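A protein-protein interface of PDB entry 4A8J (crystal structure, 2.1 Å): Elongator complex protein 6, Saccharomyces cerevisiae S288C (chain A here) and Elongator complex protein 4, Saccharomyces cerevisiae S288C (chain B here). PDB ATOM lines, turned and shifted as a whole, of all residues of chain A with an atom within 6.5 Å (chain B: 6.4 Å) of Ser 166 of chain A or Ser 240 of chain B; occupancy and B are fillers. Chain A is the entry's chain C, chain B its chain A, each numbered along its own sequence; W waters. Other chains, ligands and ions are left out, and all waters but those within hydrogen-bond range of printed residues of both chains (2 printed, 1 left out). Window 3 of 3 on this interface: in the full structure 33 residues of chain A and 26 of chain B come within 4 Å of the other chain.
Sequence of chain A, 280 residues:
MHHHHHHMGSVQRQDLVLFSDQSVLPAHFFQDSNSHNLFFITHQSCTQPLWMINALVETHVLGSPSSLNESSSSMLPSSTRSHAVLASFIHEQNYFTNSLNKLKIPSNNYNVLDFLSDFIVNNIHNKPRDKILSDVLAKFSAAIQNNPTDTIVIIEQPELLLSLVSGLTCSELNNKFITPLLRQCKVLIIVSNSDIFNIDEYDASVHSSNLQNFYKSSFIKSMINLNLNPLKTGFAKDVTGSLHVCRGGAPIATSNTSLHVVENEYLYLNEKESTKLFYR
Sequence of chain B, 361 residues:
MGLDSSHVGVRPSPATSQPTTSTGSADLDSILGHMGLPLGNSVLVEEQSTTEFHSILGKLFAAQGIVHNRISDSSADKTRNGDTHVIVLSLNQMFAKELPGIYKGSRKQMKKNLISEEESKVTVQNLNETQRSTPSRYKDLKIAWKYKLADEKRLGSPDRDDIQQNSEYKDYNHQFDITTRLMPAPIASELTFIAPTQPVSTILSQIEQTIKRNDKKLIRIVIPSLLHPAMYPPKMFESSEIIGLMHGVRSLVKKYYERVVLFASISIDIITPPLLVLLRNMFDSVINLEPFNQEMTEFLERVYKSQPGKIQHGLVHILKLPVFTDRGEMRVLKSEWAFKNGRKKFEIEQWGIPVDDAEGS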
ATOM      1  N   ILE A 120       5.927  19.672  22.394  1.00  0.00           N
ATOM      2  CA  ILE A 120       4.750  19.987  23.183  1.00  0.00           C
ATOM      3  C   ILE A 120       4.005  18.710  23.528  1.00  0.00           C
ATOM      4  O   ILE A 120       3.593  18.515  24.667  1.00  0.00           O
ATOM      5  CB  ILE A 120       3.804  20.954  22.451  1.00  0.00           C
ATOM      6  CG1 ILE A 120       4.443  22.339  22.372  1.00  0.00           C
ATOM      7  CG2 ILE A 120       2.460  21.049  23.167  1.00  0.00           C
ATOM      8  CD1 ILE A 120       4.789  22.933  23.718  1.00  0.00           C
ATOM      9  N   ILE A 124       6.030  18.264  27.345  1.00  0.00           N
ATOM     10  CA  ILE A 124       5.328  19.311  28.082  1.00  0.00           C
ATOM     11  C   ILE A 124       3.992  18.846  28.654  1.00  0.00           C
ATOM     12  O   ILE A 124       3.784  18.908  29.859  1.00  0.00           O
ATOM     13  CB  ILE A 124       5.136  20.597  27.235  1.00  0.00           C
ATOM     14  CG1 ILE A 124       6.476  21.037  26.640  1.00  0.00           C
ATOM     15  CG2 ILE A 124       4.541  21.736  28.080  1.00  0.00           C
ATOM     16  CD1 ILE A 124       6.694  22.539  26.674  1.00  0.00           C
ATOM     17  N   HIS A 125       3.104  18.371  27.788  1.00  0.00           N
ATOM     18  CA  HIS A 125       1.708  18.100  28.155  1.00  0.00           C
ATOM     19  C   HIS A 125       1.513  17.085  29.305  1.00  0.00           C
ATOM     20  O   HIS A 125       1.843  15.907  29.167  1.00  0.00           O
ATOM     21  CB  HIS A 125       0.927  17.660  26.909  1.00  0.00           C
ATOM     22  CG  HIS A 125       0.432  18.800  26.067  1.00  0.00           C
ATOM     23  ND1 HIS A 125      -0.304  18.614  24.919  1.00  0.00           N
ATOM     24  CD2 HIS A 125       0.593  20.140  26.202  1.00  0.00           C
ATOM     25  CE1 HIS A 125      -0.580  19.794  24.377  1.00  0.00           C
ATOM     26  NE2 HIS A 125      -0.049  20.730  25.138  1.00  0.00           N
ATOM     27  N   ARG A 129       6.663  21.208  35.785  1.00  0.00           N
ATOM     28  CA  ARG A 129       7.798  22.048  35.433  1.00  0.00           C
ATOM     29  C   ARG A 129       9.151  21.370  35.697  1.00  0.00           C
ATOM     30  O   ARG A 129      10.002  21.263  34.797  1.00  0.00           O
ATOM     31  CB  ARG A 129       7.693  23.361  36.206  1.00  0.00           C
ATOM     32  CG  ARG A 129       7.961  24.592  35.380  1.00  0.00           C
ATOM     33  CD  ARG A 129       7.171  25.769  35.909  1.00  0.00           C
ATOM     34  NE  ARG A 129       7.116  25.754  37.366  1.00  0.00           N
ATOM     35  CZ  ARG A 129       5.992  25.726  38.074  1.00  0.00           C
ATOM     36  NH1 ARG A 129       4.808  25.728  37.464  1.00  0.00           N
ATOM     37  NH2 ARG A 129       6.055  25.705  39.397  1.00  0.00           N
ATOM     38  N   LEU A 161      11.056  28.500  26.489  1.00  0.00           N
ATOM     39  CA  LEU A 161      10.502  27.714  27.595  1.00  0.00           C
ATOM     40  C   LEU A 161       9.669  28.580  28.530  1.00  0.00           C
ATOM     41  O   LEU A 161       8.641  28.120  29.062  1.00  0.00           O
ATOM     42  CB  LEU A 161      11.605  27.004  28.375  1.00  0.00           C
ATOM     43  CG  LEU A 161      12.159  25.759  27.663  1.00  0.00           C
ATOM     44  CD1 LEU A 161      13.431  25.274  28.314  1.00  0.00           C
ATOM     45  CD2 LEU A 161      11.092  24.639  27.645  1.00  0.00           C
ATOM     46  N   LEU A 162      10.069  29.838  28.691  1.00  0.00           N
ATOM     47  CA  LEU A 162       9.304  30.749  29.549  1.00  0.00           C
ATOM     48  C   LEU A 162       7.888  30.917  29.038  1.00  0.00           C
ATOM     49  O   LEU A 162       6.988  31.238  29.807  1.00  0.00           O
ATOM     50  CB  LEU A 162       9.982  32.114  29.660  1.00  0.00           C
ATOM     51  CG  LEU A 162      11.354  31.975  30.287  1.00  0.00           C
ATOM     52  CD1 LEU A 162      12.020  33.325  30.426  1.00  0.00           C
ATOM     53  CD2 LEU A 162      11.181  31.291  31.637  1.00  0.00           C
ATOM     54  N   SER A 163       7.680  30.704  27.736  1.00  0.00           N
ATOM     55  CA  SER A 163       6.339  30.825  27.178  1.00  0.00           C
ATOM     56  C   SER A 163       5.669  29.465  27.049  1.00  0.00           C
ATOM     57  O   SER A 163       4.442  29.368  27.071  1.00  0.00           O
ATOM     58  CB  SER A 163       6.379  31.518  25.809  1.00  0.00           C
ATOM     59  OG  SER A 163       6.814  32.863  25.931  1.00  0.00           O
ATOM     60  N   LEU A 164       6.455  28.405  26.895  1.00  0.00           N
ATOM     61  CA  LEU A 164       5.829  27.111  26.598  1.00  0.00           C
ATOM     62  C   LEU A 164       5.379  26.384  27.866  1.00  0.00           C
ATOM     63  O   LEU A 164       4.536  25.482  27.819  1.00  0.00           O
ATOM     64  CB  LEU A 164       6.770  26.206  25.813  1.00  0.00           C
ATOM     65  CG  LEU A 164       7.128  26.693  24.412  1.00  0.00           C
ATOM     66  CD1 LEU A 164       8.115  25.730  23.772  1.00  0.00           C
ATOM     67  CD2 LEU A 164       5.867  26.849  23.563  1.00  0.00           C
ATOM     68  N   VAL A 165       5.978  26.761  28.985  1.00  0.00           N
ATOM     69  CA  VAL A 165       5.791  26.053  30.238  1.00  0.00           C
ATOM     70  C   VAL A 165       5.090  26.963  31.238  1.00  0.00           C
ATOM     71  O   VAL A 165       5.640  27.975  31.683  1.00  0.00           O
ATOM     72  CB  VAL A 165       7.144  25.591  30.821  1.00  0.00           C
ATOM     73  CG1 VAL A 165       6.923  24.822  32.104  1.00  0.00           C
ATOM     74  CG2 VAL A 165       7.887  24.732  29.796  1.00  0.00           C
ATOM     75  N   SER A 166       3.856  26.597  31.566  1.00  0.00           N
ATOM     76  CA  SER A 166       3.015  27.370  32.453  1.00  0.00           C
ATOM     77  C   SER A 166       3.700  27.662  33.780  1.00  0.00           C
ATOM     78  O   SER A 166       4.176  26.757  34.459  1.00  0.00           O
ATOM     79  CB  SER A 166       1.710  26.602  32.704  1.00  0.00           C
ATOM     80  OG  SER A 166       0.758  27.412  33.365  1.00  0.00           O
ATOM     81  N   GLY A 167       3.738  28.935  34.156  1.00  0.00           N
ATOM     82  CA  GLY A 167       4.264  29.346  35.445  1.00  0.00           C
ATOM     83  C   GLY A 167       5.778  29.238  35.628  1.00  0.00           C
ATOM     84  O   GLY A 167       6.270  29.309  36.751  1.00  0.00           O
ATOM     85  N   LEU A 168       6.521  29.074  34.540  1.00  0.00           N
ATOM     86  CA  LEU A 168       7.987  29.010  34.622  1.00  0.00           C
ATOM     87  C   LEU A 168       8.610  30.411  34.755  1.00  0.00           C
ATOM     88  O   LEU A 168       8.405  31.282  33.894  1.00  0.00           O
ATOM     89  CB  LEU A 168       8.550  28.308  33.384  1.00  0.00           C
ATOM     90  CG  LEU A 168      10.064  28.074  33.397  1.00  0.00           C
ATOM     91  CD1 LEU A 168      10.458  27.270  34.634  1.00  0.00           C
ATOM     92  CD2 LEU A 168      10.515  27.379  32.129  1.00  0.00           C
ATOM     93  N   VAL B 200      -5.605  22.044  23.942  1.00  0.00           N
ATOM     94  CA  VAL B 200      -4.504  22.053  22.959  1.00  0.00           C
ATOM     95  C   VAL B 200      -4.045  20.648  22.538  1.00  0.00           C
ATOM     96  O   VAL B 200      -3.863  20.366  21.349  1.00  0.00           O
ATOM     97  CB  VAL B 200      -3.302  22.878  23.465  1.00  0.00           C
ATOM     98  CG1 VAL B 200      -2.087  22.699  22.529  1.00  0.00           C
ATOM     99  CG2 VAL B 200      -3.704  24.367  23.581  1.00  0.00           C
ATOM    100  N   PHE B 237      -5.776  32.312  25.653  1.00  0.00           N
ATOM    101  CA  PHE B 237      -4.851  33.434  25.508  1.00  0.00           C
ATOM    102  C   PHE B 237      -3.622  33.324  26.419  1.00  0.00           C
ATOM    103  O   PHE B 237      -2.681  34.115  26.301  1.00  0.00           O
ATOM    104  CB  PHE B 237      -5.570  34.768  25.739  1.00  0.00           C
ATOM    105  CG  PHE B 237      -6.380  35.245  24.558  1.00  0.00           C
ATOM    106  CD1 PHE B 237      -7.578  34.636  24.228  1.00  0.00           C
ATOM    107  CD2 PHE B 237      -5.939  36.313  23.787  1.00  0.00           C
ATOM    108  CE1 PHE B 237      -8.329  35.073  23.139  1.00  0.00           C
ATOM    109  CE2 PHE B 237      -6.685  36.766  22.702  1.00  0.00           C
ATOM    110  CZ  PHE B 237      -7.885  36.143  22.380  1.00  0.00           C
ATOM    111  N   GLU B 238      -3.626  32.358  27.329  1.00  0.00           N
ATOM    112  CA  GLU B 238      -2.425  32.086  28.103  1.00  0.00           C
ATOM    113  C   GLU B 238      -1.284  31.661  27.163  1.00  0.00           C
ATOM    114  O   GLU B 238      -1.505  30.881  26.229  1.00  0.00           O
ATOM    115  CB  GLU B 238      -2.690  30.986  29.132  1.00  0.00           C
ATOM    116  CG  GLU B 238      -3.836  31.255  30.082  1.00  0.00           C
ATOM    117  N   SER B 239      -0.067  32.148  27.412  1.00  0.00           N
ATOM    118  CA  SER B 239       1.033  31.872  26.485  1.00  0.00           C
ATOM    119  C   SER B 239       1.205  30.382  26.294  1.00  0.00           C
ATOM    120  O   SER B 239       1.300  29.911  25.169  1.00  0.00           O
ATOM    121  CB  SER B 239       2.355  32.495  26.955  1.00  0.00           C
ATOM    122  OG  SER B 239       2.293  33.914  26.905  1.00  0.00           O
ATOM    123  N   SER B 240       1.215  29.635  27.395  1.00  0.00           N
ATOM    124  CA  SER B 240       1.503  28.200  27.303  1.00  0.00           C
ATOM    125  C   SER B 240       0.448  27.496  26.472  1.00  0.00           C
ATOM    126  O   SER B 240       0.695  26.418  25.927  1.00  0.00           O
ATOM    127  CB  SER B 240       1.576  27.567  28.690  1.00  0.00           C
ATOM    128  OG  SER B 240       0.384  27.812  29.411  1.00  0.00           O
ATOM    129  N   GLU B 241      -0.743  28.097  26.396  1.00  0.00           N
ATOM    130  CA  GLU B 241      -1.846  27.534  25.619  1.00  0.00           C
ATOM    131  C   GLU B 241      -1.756  27.870  24.132  1.00  0.00           C
ATOM    132  O   GLU B 241      -1.551  26.977  23.323  1.00  0.00           O
ATOM    133  CB  GLU B 241      -3.208  27.982  26.197  1.00  0.00           C
ATOM    134  CG  GLU B 241      -3.554  27.342  27.559  1.00  0.00           C
ATOM    135  CD  GLU B 241      -3.735  25.831  27.447  1.00  0.00           C
ATOM    136  OE1 GLU B 241      -4.576  25.401  26.622  1.00  0.00           O
ATOM    137  OE2 GLU B 241      -3.024  25.076  28.152  1.00  0.00           O
ATOM    138  N   ILE B 242      -1.921  29.144  23.763  1.00  0.00           N
ATOM    139  CA  ILE B 242      -1.801  29.538  22.356  1.00  0.00           C
ATOM    140  C   ILE B 242      -0.399  29.310  21.742  1.00  0.00           C
ATOM    141  O   ILE B 242      -0.293  28.801  20.627  1.00  0.00           O
ATOM    142  CB  ILE B 242      -2.263  31.001  22.114  1.00  0.00           C
ATOM    143  CG1 ILE B 242      -2.063  31.393  20.648  1.00  0.00           C
ATOM    144  CG2 ILE B 242      -1.521  31.954  23.016  1.00  0.00           C
ATOM    145  CD1 ILE B 242      -2.956  30.642  19.675  1.00  0.00           C
ATOM    146  N   ILE B 243       0.662  29.682  22.456  1.00  0.00           N
ATOM    147  CA  ILE B 243       2.010  29.470  21.924  1.00  0.00           C
ATOM    148  C   ILE B 243       2.381  27.971  21.903  1.00  0.00           C
ATOM    149  O   ILE B 243       3.003  27.484  20.955  1.00  0.00           O
ATOM    150  CB  ILE B 243       3.081  30.333  22.652  1.00  0.00           C
ATOM    151  CG1 ILE B 243       2.740  31.824  22.506  1.00  0.00           C
ATOM    152  CG2 ILE B 243       4.479  30.059  22.070  1.00  0.00           C
ATOM    153  CD1 ILE B 243       2.422  32.253  21.045  1.00  0.00           C
ATOM    154  N   GLY B 244       1.982  27.226  22.928  1.00  0.00           N
ATOM    155  CA  GLY B 244       2.093  25.776  22.854  1.00  0.00           C
ATOM    156  C   GLY B 244       1.435  25.249  21.590  1.00  0.00           C
ATOM    157  O   GLY B 244       2.061  24.539  20.789  1.00  0.00           O
ATOM    158  N   LEU B 245       0.176  25.625  21.375  1.00  0.00           N
ATOM    159  CA  LEU B 245      -0.540  25.225  20.155  1.00  0.00           C
ATOM    160  C   LEU B 245       0.272  25.533  18.894  1.00  0.00           C
ATOM    161  O   LEU B 245       0.571  24.635  18.096  1.00  0.00           O
ATOM    162  CB  LEU B 245      -1.924  25.903  20.070  1.00  0.00           C
ATOM    163  CG  LEU B 245      -2.774  25.645  18.813  1.00  0.00           C
ATOM    164  CD1 LEU B 245      -2.987  24.154  18.585  1.00  0.00           C
ATOM    165  CD2 LEU B 245      -4.156  26.391  18.837  1.00  0.00           C
HETATM  166  O   HOH W   1      -1.245  28.960  31.635  1.00  0.00           O
HETATM  167  O   HOH W   2       2.407  24.400  26.430  1.00  0.00           O
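The backbone carbonyl oxygen (O) of Ile 120 of chain A is in hydrogen-bond range of the backbone NH (N) of His 125 of chain A, 3.2 Å away. NH1 of Arg 129 of chain A is in hydrogen-bond range of O of Ser 166 of chain A, at 3.2 Å.
Printed residues of chain B that touch a printed residue of chain A: Val 200, Ser 239, Ser 240, Ile 243 and Gly 244. Hydrophobic or aromatic side chains of chain B that line the printed part of chain A: Val 200 and Ile 243. Hydrophobic or aromatic side chains of chain A that line the printed part of chain B: Ile 120, His 125 and Leu 164. Among the printed residues, 8 pairs touch across the chains. Among the printed residues, no Asp or Glu carboxylate lies within 4 Å of a Lys or Arg side-chain nitrogen of the other chain.
N of Ser 240 of chain B sits close to O of Ser 163 of chain A, at 3.3 Å.
Of the printed residues of chain B, Leu 164 of chain A touches Ser 240 (3.7 Å), Ile 243 (3.8 Å) and Gly 244 (3.95 Å). Ser 166 of chain A touches just one residue of chain B: Ser 240. Printed residues of chain A within 4 Å of Val 200 of chain B: His 125 (3.8 Å). Printed residues of chain A within 4 Å of Ser 239 of chain B: Ser 163 (3.5 Å). Of chain A, only Ser 163, Leu 164 and Ser 166 come within 4 Å of Ser 240 of chain B. Ile 242 of chain B touches none of the printed residues of chain A. Printed residues of chain A within 4 Å of Ile 243 of chain B: Leu 164 (3.8 Å). The nearest printed residue of chain B that does not touch Ser 166 of chain A is Glu 238 of chain B (6.5 Å). The nearest residue of chain A that does not touch Ser 240 of chain B is Val 165 of chain A (4.4 Å). The nearest printed residue of chain A that does not touch Gly 244 of chain B is Ser 163 of chain A (5.3 Å).
O of Gly 244 of chain B touches CG1 of Ile 120 of chain A (3.6 Å). Val 200 of chain B touches His 125 of chain A. Ser 239 of chain B touches Ser 163 of chain A (C to O, 3.5 Å). Ser 240 of chain B touches Leu 164 of chain A (CB to O, 3.7 Å). Leu 164 of chain A touches Ile 243 of chain B (CD2 to CG2, 3.8 Å). Leu 164 of chain A touches Gly 244 of chain B. Ser 166 of chain A touches Ser 240 of chain B.
Water W2 lies within hydrogen-bond range of O of Ser 240 of chain B (2.7 Å) and O of Leu 164 of chain A (2.8 Å). Water W1 lies within hydrogen-bond range of the side-chain hydroxyl (OG) of Ser 240 of chain B and the side-chain hydroxyl (OG) of Ser 166 of chain A.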
